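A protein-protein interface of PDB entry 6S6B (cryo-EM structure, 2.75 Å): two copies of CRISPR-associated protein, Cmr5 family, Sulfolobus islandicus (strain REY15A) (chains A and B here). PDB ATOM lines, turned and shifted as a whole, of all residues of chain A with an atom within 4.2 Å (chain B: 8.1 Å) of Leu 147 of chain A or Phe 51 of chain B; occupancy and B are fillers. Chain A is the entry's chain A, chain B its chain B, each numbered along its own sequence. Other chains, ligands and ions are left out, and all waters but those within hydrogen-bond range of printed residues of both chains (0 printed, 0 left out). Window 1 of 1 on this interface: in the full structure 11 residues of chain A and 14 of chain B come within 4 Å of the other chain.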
ATOM      1  N   TYR A   7      13.254  -9.585  10.221  1.00  0.00           N
ATOM      2  CA  TYR A   7      13.900  -8.631  11.111  1.00  0.00           C
ATOM      3  C   TYR A   7      15.303  -9.080  11.473  1.00  0.00           C
ATOM      4  O   TYR A   7      16.179  -8.243  11.704  1.00  0.00           O
ATOM      5  CB  TYR A   7      13.068  -8.431  12.375  1.00  0.00           C
ATOM      6  CG  TYR A   7      11.983  -7.403  12.214  1.00  0.00           C
ATOM      7  CD1 TYR A   7      10.804  -7.712  11.561  1.00  0.00           C
ATOM      8  CD2 TYR A   7      12.142  -6.121  12.704  1.00  0.00           C
ATOM      9  CE1 TYR A   7       9.812  -6.778  11.407  1.00  0.00           C
ATOM     10  CE2 TYR A   7      11.156  -5.176  12.553  1.00  0.00           C
ATOM     11  CZ  TYR A   7       9.993  -5.510  11.903  1.00  0.00           C
ATOM     12  OH  TYR A   7       9.004  -4.570  11.748  1.00  0.00           O
ATOM     13  N   ALA A  10      17.281  -8.358   8.271  1.00  0.00           N
ATOM     14  CA  ALA A  10      17.605  -6.943   8.216  1.00  0.00           C
ATOM     15  C   ALA A  10      18.707  -6.565   9.189  1.00  0.00           C
ATOM     16  O   ALA A  10      19.291  -5.488   9.053  1.00  0.00           O
ATOM     17  CB  ALA A  10      16.359  -6.111   8.501  1.00  0.00           C
ATOM     18  N   LEU A  11      18.996  -7.409  10.176  1.00  0.00           N
ATOM     19  CA  LEU A  11      20.105  -7.127  11.077  1.00  0.00           C
ATOM     20  C   LEU A  11      21.435  -7.510  10.453  1.00  0.00           C
ATOM     21  O   LEU A  11      22.415  -6.770  10.572  1.00  0.00           O
ATOM     22  CB  LEU A  11      19.907  -7.854  12.401  1.00  0.00           C
ATOM     23  CG  LEU A  11      19.286  -7.008  13.508  1.00  0.00           C
ATOM     24  CD1 LEU A  11      18.800  -7.888  14.636  1.00  0.00           C
ATOM     25  CD2 LEU A  11      20.291  -5.999  14.017  1.00  0.00           C
ATOM     26  N   PHE A  14      22.029  -4.819   7.504  1.00  0.00           N
ATOM     27  CA  PHE A  14      22.435  -3.513   8.005  1.00  0.00           C
ATOM     28  C   PHE A  14      23.815  -3.560   8.634  1.00  0.00           C
ATOM     29  O   PHE A  14      24.550  -2.571   8.583  1.00  0.00           O
ATOM     30  CB  PHE A  14      21.422  -2.991   9.015  1.00  0.00           C
ATOM     31  CG  PHE A  14      21.800  -1.676   9.619  1.00  0.00           C
ATOM     32  CD1 PHE A  14      21.539  -0.498   8.954  1.00  0.00           C
ATOM     33  CD2 PHE A  14      22.411  -1.617  10.851  1.00  0.00           C
ATOM     34  CE1 PHE A  14      21.885   0.708   9.508  1.00  0.00           C
ATOM     35  CE2 PHE A  14      22.756  -0.409  11.406  1.00  0.00           C
ATOM     36  CZ  PHE A  14      22.492   0.751  10.733  1.00  0.00           C
ATOM     37  N   ALA A 143      12.170  -2.500   8.360  1.00  0.00           N
ATOM     38  CA  ALA A 143      13.109  -2.763   9.443  1.00  0.00           C
ATOM     39  C   ALA A 143      14.425  -2.039   9.203  1.00  0.00           C
ATOM     40  O   ALA A 143      14.983  -1.427  10.119  1.00  0.00           O
ATOM     41  CB  ALA A 143      13.337  -4.265   9.584  1.00  0.00           C
ATOM     42  N   ILE A 144      14.938  -2.109   7.972  1.00  0.00           N
ATOM     43  CA  ILE A 144      16.125  -1.347   7.598  1.00  0.00           C
ATOM     44  C   ILE A 144      15.923   0.131   7.886  1.00  0.00           C
ATOM     45  O   ILE A 144      16.838   0.823   8.341  1.00  0.00           O
ATOM     46  CB  ILE A 144      16.462  -1.579   6.116  1.00  0.00           C
ATOM     47  CG1 ILE A 144      16.817  -3.038   5.860  1.00  0.00           C
ATOM     48  CG2 ILE A 144      17.589  -0.677   5.681  1.00  0.00           C
ATOM     49  CD1 ILE A 144      18.066  -3.471   6.549  1.00  0.00           C
ATOM     50  N   LYS A 145      14.719   0.638   7.629  1.00  0.00           N
ATOM     51  CA  LYS A 145      14.458   2.052   7.847  1.00  0.00           C
ATOM     52  C   LYS A 145      14.565   2.418   9.314  1.00  0.00           C
ATOM     53  O   LYS A 145      14.917   3.551   9.646  1.00  0.00           O
ATOM     54  CB  LYS A 145      13.076   2.417   7.318  1.00  0.00           C
ATOM     55  CG  LYS A 145      12.754   3.882   7.450  1.00  0.00           C
ATOM     56  CD  LYS A 145      11.273   4.128   7.544  1.00  0.00           C
ATOM     57  CE  LYS A 145      11.010   5.462   8.210  1.00  0.00           C
ATOM     58  NZ  LYS A 145       9.563   5.754   8.345  1.00  0.00           N
ATOM     59  N   ARG A 146      14.281   1.479  10.204  1.00  0.00           N
ATOM     60  CA  ARG A 146      14.284   1.777  11.624  1.00  0.00           C
ATOM     61  C   ARG A 146      15.638   1.544  12.269  1.00  0.00           C
ATOM     62  O   ARG A 146      16.001   2.265  13.204  1.00  0.00           O
ATOM     63  CB  ARG A 146      13.216   0.944  12.325  1.00  0.00           C
ATOM     64  CG  ARG A 146      11.840   1.173  11.762  1.00  0.00           C
ATOM     65  CD  ARG A 146      10.833   0.286  12.436  1.00  0.00           C
ATOM     66  NE  ARG A 146       9.519   0.338  11.811  1.00  0.00           N
ATOM     67  CZ  ARG A 146       8.714   1.393  11.840  1.00  0.00           C
ATOM     68  NH1 ARG A 146       9.089   2.502  12.459  1.00  0.00           N
ATOM     69  NH2 ARG A 146       7.533   1.339  11.246  1.00  0.00           N
ATOM     70  N   LEU A 147      16.394   0.552  11.801  1.00  0.00           N
ATOM     71  CA  LEU A 147      17.782   0.436  12.225  1.00  0.00           C
ATOM     72  C   LEU A 147      18.582   1.646  11.778  1.00  0.00           C
ATOM     73  O   LEU A 147      19.437   2.144  12.516  1.00  0.00           O
ATOM     74  CB  LEU A 147      18.400  -0.841  11.670  1.00  0.00           C
ATOM     75  CG  LEU A 147      17.988  -2.130  12.360  1.00  0.00           C
ATOM     76  CD1 LEU A 147      18.716  -3.296  11.739  1.00  0.00           C
ATOM     77  CD2 LEU A 147      18.274  -2.036  13.840  1.00  0.00           C
ATOM     78  N   SER A 148      18.320   2.127  10.567  1.00  0.00           N
ATOM     79  CA  SER A 148      19.010   3.309  10.071  1.00  0.00           C
ATOM     80  C   SER A 148      18.742   4.510  10.960  1.00  0.00           C
ATOM     81  O   SER A 148      19.672   5.196  11.391  1.00  0.00           O
ATOM     82  CB  SER A 148      18.576   3.590   8.639  1.00  0.00           C
ATOM     83  OG  SER A 148      18.916   2.507   7.800  1.00  0.00           O
ATOM     84  N   GLU A 149      17.473   4.778  11.252  1.00  0.00           N
ATOM     85  CA  GLU A 149      17.133   5.918  12.089  1.00  0.00           C
ATOM     86  C   GLU A 149      17.613   5.756  13.523  1.00  0.00           C
ATOM     87  O   GLU A 149      17.671   6.744  14.260  1.00  0.00           O
ATOM     88  CB  GLU A 149      15.626   6.145  12.071  1.00  0.00           C
ATOM     89  CG  GLU A 149      15.089   6.515  10.710  1.00  0.00           C
ATOM     90  CD  GLU A 149      13.600   6.783  10.725  1.00  0.00           C
ATOM     91  OE1 GLU A 149      12.829   5.860  11.060  1.00  0.00           O
ATOM     92  OE2 GLU A 149      13.201   7.922  10.397  1.00  0.00           O
ATOM     93  N   ALA A 150      17.953   4.541  13.937  1.00  0.00           N
ATOM     94  CA  ALA A 150      18.389   4.290  15.302  1.00  0.00           C
ATOM     95  C   ALA A 150      19.903   4.282  15.431  1.00  0.00           C
ATOM     96  O   ALA A 150      20.455   4.935  16.318  1.00  0.00           O
ATOM     97  CB  ALA A 150      17.821   2.958  15.797  1.00  0.00           C
ATOM     98  N   LEU A 151      20.586   3.558  14.553  1.00  0.00           N
ATOM     99  CA  LEU A 151      22.020   3.367  14.676  1.00  0.00           C
ATOM    100  C   LEU A 151      22.830   4.467  14.014  1.00  0.00           C
ATOM    101  O   LEU A 151      24.026   4.585  14.293  1.00  0.00           O
ATOM    102  CB  LEU A 151      22.423   2.018  14.078  1.00  0.00           C
ATOM    103  CG  LEU A 151      22.259   0.777  14.956  1.00  0.00           C
ATOM    104  CD1 LEU A 151      23.084   0.922  16.214  1.00  0.00           C
ATOM    105  CD2 LEU A 151      20.808   0.491  15.292  1.00  0.00           C
ATOM    106  N   GLY B  45       4.497  -7.920  17.944  1.00  0.00           N
ATOM    107  CA  GLY B  45       5.673  -8.635  18.389  1.00  0.00           C
ATOM    108  C   GLY B  45       6.625  -7.730  19.147  1.00  0.00           C
ATOM    109  O   GLY B  45       6.518  -6.504  19.135  1.00  0.00           O
ATOM    110  N   PHE B  46       7.585  -8.366  19.814  1.00  0.00           N
ATOM    111  CA  PHE B  46       8.488  -7.611  20.672  1.00  0.00           C
ATOM    112  C   PHE B  46       9.504  -6.830  19.854  1.00  0.00           C
ATOM    113  O   PHE B  46       9.594  -5.604  19.964  1.00  0.00           O
ATOM    114  CB  PHE B  46       9.198  -8.537  21.652  1.00  0.00           C
ATOM    115  CG  PHE B  46      10.258  -7.851  22.446  1.00  0.00           C
ATOM    116  CD1 PHE B  46       9.922  -6.984  23.460  1.00  0.00           C
ATOM    117  CD2 PHE B  46      11.592  -8.053  22.163  1.00  0.00           C
ATOM    118  CE1 PHE B  46      10.894  -6.342  24.182  1.00  0.00           C
ATOM    119  CE2 PHE B  46      12.566  -7.414  22.882  1.00  0.00           C
ATOM    120  CZ  PHE B  46      12.218  -6.557  23.892  1.00  0.00           C
ATOM    121  N   ILE B  47      10.288  -7.518  19.033  1.00  0.00           N
ATOM    122  CA  ILE B  47      11.357  -6.835  18.312  1.00  0.00           C
ATOM    123  C   ILE B  47      10.817  -5.925  17.210  1.00  0.00           C
ATOM    124  O   ILE B  47      11.428  -4.876  16.969  1.00  0.00           O
ATOM    125  CB  ILE B  47      12.404  -7.821  17.765  1.00  0.00           C
ATOM    126  CG1 ILE B  47      11.774  -8.968  16.999  1.00  0.00           C
ATOM    127  CG2 ILE B  47      13.251  -8.369  18.891  1.00  0.00           C
ATOM    128  CD1 ILE B  47      12.627  -9.438  15.879  1.00  0.00           C
ATOM    129  N   PRO B  48       9.711  -6.233  16.517  1.00  0.00           N
ATOM    130  CA  PRO B  48       9.149  -5.209  15.629  1.00  0.00           C
ATOM    131  C   PRO B  48       8.799  -3.935  16.360  1.00  0.00           C
ATOM    132  O   PRO B  48       8.945  -2.845  15.797  1.00  0.00           O
ATOM    133  CB  PRO B  48       7.906  -5.895  15.056  1.00  0.00           C
ATOM    134  CG  PRO B  48       8.238  -7.306  15.096  1.00  0.00           C
ATOM    135  CD  PRO B  48       8.935  -7.478  16.392  1.00  0.00           C
ATOM    136  N   THR B  49       8.349  -4.039  17.606  1.00  0.00           N
ATOM    137  CA  THR B  49       8.103  -2.855  18.410  1.00  0.00           C
ATOM    138  C   THR B  49       9.386  -2.301  19.000  1.00  0.00           C
ATOM    139  O   THR B  49       9.486  -1.093  19.229  1.00  0.00           O
ATOM    140  CB  THR B  49       7.127  -3.178  19.530  1.00  0.00           C
ATOM    141  OG1 THR B  49       6.081  -4.005  19.013  1.00  0.00           O
ATOM    142  CG2 THR B  49       6.529  -1.906  20.086  1.00  0.00           C
ATOM    143  N   PHE B  50      10.368  -3.162  19.260  1.00  0.00           N
ATOM    144  CA  PHE B  50      11.647  -2.680  19.758  1.00  0.00           C
ATOM    145  C   PHE B  50      12.353  -1.840  18.706  1.00  0.00           C
ATOM    146  O   PHE B  50      12.879  -0.764  19.008  1.00  0.00           O
ATOM    147  CB  PHE B  50      12.522  -3.853  20.185  1.00  0.00           C
ATOM    148  CG  PHE B  50      13.739  -3.442  20.938  1.00  0.00           C
ATOM    149  CD1 PHE B  50      13.645  -3.036  22.254  1.00  0.00           C
ATOM    150  CD2 PHE B  50      14.976  -3.443  20.331  1.00  0.00           C
ATOM    151  CE1 PHE B  50      14.762  -2.650  22.951  1.00  0.00           C
ATOM    152  CE2 PHE B  50      16.094  -3.057  21.023  1.00  0.00           C
ATOM    153  CZ  PHE B  50      15.988  -2.659  22.335  1.00  0.00           C
ATOM    154  N   PHE B  51      12.375  -2.322  17.460  1.00  0.00           N
ATOM    155  CA  PHE B  51      12.921  -1.532  16.364  1.00  0.00           C
ATOM    156  C   PHE B  51      12.229  -0.184  16.273  1.00  0.00           C
ATOM    157  O   PHE B  51      12.877   0.857  16.135  1.00  0.00           O
ATOM    158  CB  PHE B  51      12.769  -2.288  15.047  1.00  0.00           C
ATOM    159  CG  PHE B  51      13.839  -3.298  14.797  1.00  0.00           C
ATOM    160  CD1 PHE B  51      14.284  -4.122  15.807  1.00  0.00           C
ATOM    161  CD2 PHE B  51      14.389  -3.438  13.542  1.00  0.00           C
ATOM    162  CE1 PHE B  51      15.256  -5.055  15.570  1.00  0.00           C
ATOM    163  CE2 PHE B  51      15.363  -4.369  13.303  1.00  0.00           C
ATOM    164  CZ  PHE B  51      15.797  -5.178  14.317  1.00  0.00           C
ATOM    165  N   TYR B  52      10.901  -0.187  16.348  1.00  0.00           N
ATOM    166  CA  TYR B  52      10.153   1.059  16.314  1.00  0.00           C
ATOM    167  C   TYR B  52      10.524   1.966  17.475  1.00  0.00           C
ATOM    168  O   TYR B  52      10.536   3.190  17.324  1.00  0.00           O
ATOM    169  CB  TYR B  52       8.660   0.751  16.332  1.00  0.00           C
ATOM    170  CG  TYR B  52       7.763   1.957  16.294  1.00  0.00           C
ATOM    171  CD1 TYR B  52       7.310   2.466  15.093  1.00  0.00           C
ATOM    172  CD2 TYR B  52       7.345   2.568  17.460  1.00  0.00           C
ATOM    173  CE1 TYR B  52       6.489   3.558  15.049  1.00  0.00           C
ATOM    174  CE2 TYR B  52       6.522   3.660  17.427  1.00  0.00           C
ATOM    175  CZ  TYR B  52       6.096   4.151  16.218  1.00  0.00           C
ATOM    176  OH  TYR B  52       5.268   5.245  16.180  1.00  0.00           O
ATOM    177  N   ILE B  53      10.829   1.393  18.638  1.00  0.00           N
ATOM    178  CA  ILE B  53      11.140   2.211  19.803  1.00  0.00           C
ATOM    179  C   ILE B  53      12.482   2.902  19.627  1.00  0.00           C
ATOM    180  O   ILE B  53      12.602   4.115  19.824  1.00  0.00           O
ATOM    181  CB  ILE B  53      11.109   1.360  21.084  1.00  0.00           C
ATOM    182  CG1 ILE B  53       9.670   1.074  21.491  1.00  0.00           C
ATOM    183  CG2 ILE B  53      11.804   2.075  22.217  1.00  0.00           C
ATOM    184  CD1 ILE B  53       9.550   0.049  22.571  1.00  0.00           C
ATOM    185  N   ILE B  54      13.512   2.145  19.249  1.00  0.00           N
ATOM    186  CA  ILE B  54      14.842   2.731  19.141  1.00  0.00           C
ATOM    187  C   ILE B  54      14.899   3.715  17.983  1.00  0.00           C
ATOM    188  O   ILE B  54      15.579   4.742  18.060  1.00  0.00           O
ATOM    189  CB  ILE B  54      15.913   1.633  19.005  1.00  0.00           C
ATOM    190  CG1 ILE B  54      15.517   0.618  17.941  1.00  0.00           C
ATOM    191  CG2 ILE B  54      16.121   0.934  20.323  1.00  0.00           C
ATOM    192  CD1 ILE B  54      16.591  -0.387  17.642  1.00  0.00           C
ATOM    193  N   SER B  55      14.182   3.426  16.897  1.00  0.00           N
ATOM    194  CA  SER B  55      14.184   4.327  15.751  1.00  0.00           C
ATOM    195  C   SER B  55      13.598   5.683  16.113  1.00  0.00           C
ATOM    196  O   SER B  55      14.053   6.717  15.614  1.00  0.00           O
ATOM    197  CB  SER B  55      13.414   3.703  14.594  1.00  0.00           C
ATOM    198  OG  SER B  55      12.040   3.604  14.900  1.00  0.00           O
ATOM    199  N   LYS B  56      12.590   5.702  16.974  1.00  0.00           N
ATOM    200  CA  LYS B  56      12.024   6.952  17.457  1.00  0.00           C
ATOM    201  C   LYS B  56      12.748   7.494  18.675  1.00  0.00           C
ATOM    202  O   LYS B  56      12.514   8.645  19.052  1.00  0.00           O
ATOM    203  CB  LYS B  56      10.546   6.770  17.801  1.00  0.00           C
ATOM    204  CG  LYS B  56       9.677   6.335  16.649  1.00  0.00           C
ATOM    205  CD  LYS B  56       9.180   7.530  15.877  1.00  0.00           C
ATOM    206  CE  LYS B  56       7.985   7.177  15.028  1.00  0.00           C
ATOM    207  NZ  LYS B  56       6.743   7.154  15.835  1.00  0.00           N
ATOM    208  N   ALA B  57      13.608   6.700  19.308  1.00  0.00           N
ATOM    209  CA  ALA B  57      14.293   7.154  20.508  1.00  0.00           C
ATOM    210  C   ALA B  57      15.424   8.115  20.190  1.00  0.00           C
ATOM    211  O   ALA B  57      15.752   8.967  21.023  1.00  0.00           O
ATOM    212  CB  ALA B  57      14.832   5.960  21.291  1.00  0.00           C
ATOM    213  N   ASN B  60      22.430   7.700  20.580  1.00  0.00           N
ATOM    214  CA  ASN B  60      23.732   8.218  20.176  1.00  0.00           C
ATOM    215  C   ASN B  60      23.863   9.696  20.533  1.00  0.00           C
ATOM    216  O   ASN B  60      24.003  10.566  19.675  1.00  0.00           O
ATOM    217  CB  ASN B  60      23.962   7.997  18.679  1.00  0.00           C
ATOM    218  CG  ASN B  60      23.737   6.563  18.260  1.00  0.00           C
ATOM    219  OD1 ASN B  60      22.875   6.271  17.431  1.00  0.00           O
ATOM    220  ND2 ASN B  60      24.489   5.655  18.857  1.00  0.00           N
ATOM    221  N   TYR B  87      10.004   8.283  24.108  1.00  0.00           N
ATOM    222  CA  TYR B  87      10.340   6.994  23.516  1.00  0.00           C
ATOM    223  C   TYR B  87      11.599   6.416  24.139  1.00  0.00           C
ATOM    224  O   TYR B  87      11.718   5.198  24.292  1.00  0.00           O
ATOM    225  CB  TYR B  87      10.507   7.135  22.010  1.00  0.00           C
ATOM    226  CG  TYR B  87       9.249   6.847  21.245  1.00  0.00           C
ATOM    227  CD1 TYR B  87       8.779   5.554  21.113  1.00  0.00           C
ATOM    228  CD2 TYR B  87       8.523   7.869  20.667  1.00  0.00           C
ATOM    229  CE1 TYR B  87       7.628   5.289  20.419  1.00  0.00           C
ATOM    230  CE2 TYR B  87       7.374   7.615  19.973  1.00  0.00           C
ATOM    231  CZ  TYR B  87       6.929   6.324  19.853  1.00  0.00           C
ATOM    232  OH  TYR B  87       5.773   6.072  19.157  1.00  0.00           O
ATOM    233  N   LEU B  91      12.364   3.003  26.452  1.00  0.00           N
ATOM    234  CA  LEU B  91      13.459   2.075  26.212  1.00  0.00           C
ATOM    235  C   LEU B  91      14.166   1.733  27.511  1.00  0.00           C
ATOM    236  O   LEU B  91      14.602   0.595  27.708  1.00  0.00           O
ATOM    237  CB  LEU B  91      14.440   2.671  25.207  1.00  0.00           C
ATOM    238  CG  LEU B  91      15.636   1.794  24.856  1.00  0.00           C
ATOM    239  CD1 LEU B  91      15.156   0.460  24.354  1.00  0.00           C
ATOM    240  CD2 LEU B  91      16.496   2.470  23.821  1.00  0.00           C
ATOM    241  N   ARG B 119      26.183  -2.345  19.843  1.00  0.00           N
ATOM    242  CA  ARG B 119      24.731  -2.195  19.857  1.00  0.00           C
ATOM    243  C   ARG B 119      24.066  -3.191  18.923  1.00  0.00           C
ATOM    244  O   ARG B 119      23.008  -3.739  19.246  1.00  0.00           O
ATOM    245  CB  ARG B 119      24.335  -0.773  19.477  1.00  0.00           C
ATOM    246  CG  ARG B 119      25.088   0.281  20.229  1.00  0.00           C
ATOM    247  CD  ARG B 119      24.197   1.444  20.580  1.00  0.00           C
ATOM    248  NE  ARG B 119      24.976   2.537  21.140  1.00  0.00           N
ATOM    249  CZ  ARG B 119      25.744   3.338  20.415  1.00  0.00           C
ATOM    250  NH1 ARG B 119      25.831   3.162  19.105  1.00  0.00           N
ATOM    251  NH2 ARG B 119      26.425   4.314  20.995  1.00  0.00           N
ATOM    252  N   LEU B 120      24.670  -3.443  17.764  1.00  0.00           N
ATOM    253  CA  LEU B 120      24.130  -4.455  16.868  1.00  0.00           C
ATOM    254  C   LEU B 120      24.115  -5.826  17.521  1.00  0.00           C
ATOM    255  O   LEU B 120      23.238  -6.644  17.227  1.00  0.00           O
ATOM    256  CB  LEU B 120      24.938  -4.497  15.574  1.00  0.00           C
ATOM    257  CG  LEU B 120      24.861  -3.240  14.717  1.00  0.00           C
ATOM    258  CD1 LEU B 120      25.288  -3.550  13.298  1.00  0.00           C
ATOM    259  CD2 LEU B 120      23.456  -2.681  14.745  1.00  0.00           C
ATOM    260  N   ILE B 123      20.951  -5.836  19.844  1.00  0.00           N
ATOM    261  CA  ILE B 123      19.759  -6.147  19.066  1.00  0.00           C
ATOM    262  C   ILE B 123      19.786  -7.592  18.598  1.00  0.00           C
ATOM    263  O   ILE B 123      18.740  -8.229  18.457  1.00  0.00           O
ATOM    264  CB  ILE B 123      19.621  -5.184  17.872  1.00  0.00           C
ATOM    265  CG1 ILE B 123      20.030  -3.765  18.259  1.00  0.00           C
ATOM    266  CG2 ILE B 123      18.204  -5.186  17.366  1.00  0.00           C
ATOM    267  CD1 ILE B 123      19.137  -3.130  19.269  1.00  0.00           C
ATOM    268  N   ASP B 124      20.976  -8.130  18.347  1.00  0.00           N
ATOM    269  CA  ASP B 124      21.077  -9.525  17.948  1.00  0.00           C
ATOM    270  C   ASP B 124      20.800 -10.458  19.116  1.00  0.00           C
ATOM    271  O   ASP B 124      20.281 -11.559  18.918  1.00  0.00           O
ATOM    272  CB  ASP B 124      22.461  -9.795  17.368  1.00  0.00           C
ATOM    273  CG  ASP B 124      22.511 -11.061  16.556  1.00  0.00           C
ATOM    274  OD1 ASP B 124      21.472 -11.743  16.455  1.00  0.00           O
ATOM    275  OD2 ASP B 124      23.591 -11.375  16.013  1.00  0.00           O
ATOM    276  N   LEU B 126      18.720  -9.670  21.716  1.00  0.00           N
ATOM    277  CA  LEU B 126      17.298  -9.564  22.005  1.00  0.00           C
ATOM    278  C   LEU B 126      16.459 -10.336  21.006  1.00  0.00           C
ATOM    279  O   LEU B 126      15.343 -10.750  21.328  1.00  0.00           O
ATOM    280  CB  LEU B 126      16.870  -8.103  22.023  1.00  0.00           C
ATOM    281  CG  LEU B 126      17.483  -7.293  23.153  1.00  0.00           C
ATOM    282  CD1 LEU B 126      16.866  -5.919  23.207  1.00  0.00           C
ATOM    283  CD2 LEU B 126      17.291  -8.021  24.455  1.00  0.00           C
ATOM    284  N   TYR B 127      16.962 -10.534  19.792  1.00  0.00           N
ATOM    285  CA  TYR B 127      16.187 -11.272  18.806  1.00  0.00           C
ATOM    286  C   TYR B 127      15.994 -12.720  19.232  1.00  0.00           C
ATOM    287  O   TYR B 127      14.923 -13.296  19.022  1.00  0.00           O
ATOM    288  CB  TYR B 127      16.859 -11.207  17.440  1.00  0.00           C
ATOM    289  CG  TYR B 127      16.240 -12.150  16.442  1.00  0.00           C
ATOM    290  CD1 TYR B 127      15.067 -11.820  15.790  1.00  0.00           C
ATOM    291  CD2 TYR B 127      16.822 -13.372  16.162  1.00  0.00           C
ATOM    292  CE1 TYR B 127      14.494 -12.674  14.887  1.00  0.00           C
ATOM    293  CE2 TYR B 127      16.255 -14.233  15.259  1.00  0.00           C
ATOM    294  CZ  TYR B 127      15.092 -13.881  14.623  1.00  0.00           C
ATOM    295  OH  TYR B 127      14.525 -14.745  13.719  1.00  0.00           O
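The backbone carbonyl oxygen (O) of Ala 150 of chain A sits close to the side-chain amide oxygen (OD1) of Asn 60 of chain B, 3.0 Å away.
The side-chain hydroxyl of Tyr 52 of chain B lies within hydrogen-bond range of the side-chain amino group of Lys 56 of chain B.
ND2 of Asn 60 of chain B lies close to NH1 of Arg 119 of chain B, 2.8 Å away.
The backbone carbonyl oxygen (O) of Tyr 52 of chain B sits at hydrogen-bond distance from the side-chain hydroxyl (OG) of Ser 55 of chain B (2.9 Å).
The side-chain hydroxyl (OH) of Tyr 87 of chain B lies close to the side-chain hydroxyl (OH) of Tyr 52 of chain B.
The backbone carbonyl oxygen (O) of Phe 51 of chain B is in hydrogen-bond range of the side-chain hydroxyl (OG) of Ser 55 of chain B, 3.1 Å away.
Tyr 7 of chain A touches Pro 48 of chain B (CE2 to CA, 3.7 Å).
Phe 51 of chain B touches Tyr 7 of chain A (CD2 to CD2, 3.6 Å).
Ile 123 of chain B touches Leu 11 of chain A (O to CD1, 3.8 Å).
Arg 146 of chain A touches Phe 51 of chain B.
Arg 146 of chain A touches Tyr 52 of chain B (NH1 to CD1, 3.2 Å).
Phe 51 of chain B touches Leu 147 of chain A (CE2 to CG, 3.6 Å).
O of Glu 149 of chain A touches O of Ser 55 of chain B (3.9 Å).
Ser 55 of chain B touches Ala 150 of chain A.
CD1 of Leu 151 of chain A touches CB of Arg 119 of chain B (3.9 Å).
CG of Leu 151 of chain A touches CD2 of Leu 120 of chain B (3.7 Å).
Printed residues of chain B within 4 Å of Tyr 7 of chain A: Ile 47, Pro 48 and Phe 51.
Of the printed residues of chain B, Arg 146 of chain A touches Phe 51, Tyr 52 and Ser 55.
Of chain B, only Phe 51 (3.6 Å) comes within 4 Å of Leu 147 of chain A.
Of the printed residues of chain A, Ile 54 of chain B touches Ala 150 (3.7 Å).
Of the printed residues of chain A, Asn 60 of chain B touches Ala 150 and Leu 151.
Printed residues of chain A within 4 Å of Leu 120 of chain B: Leu 151.
The nearest residue of chain B that does not touch Leu 147 of chain A is Ile 54 of chain B (4.5 Å).
Of the 13 printed residues of chain A, 7 touch a printed residue of chain B.
Hydrophobic or aromatic side chains of chain A that line the printed part of chain B: Tyr 7, Leu 11, Leu 147, Ala 150 and Leu 151.
Among the printed residues, 15 pairs touch across the chains.
Among the printed residues, no Asp or Glu carboxylate lies within 4 Å of a Lys or Arg side-chain nitrogen of the other chain.
No position is printed for both chains.
Of the 15 pairs that touch across the chains among the printed residues, none has its exchanged pair printed and touching as well.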
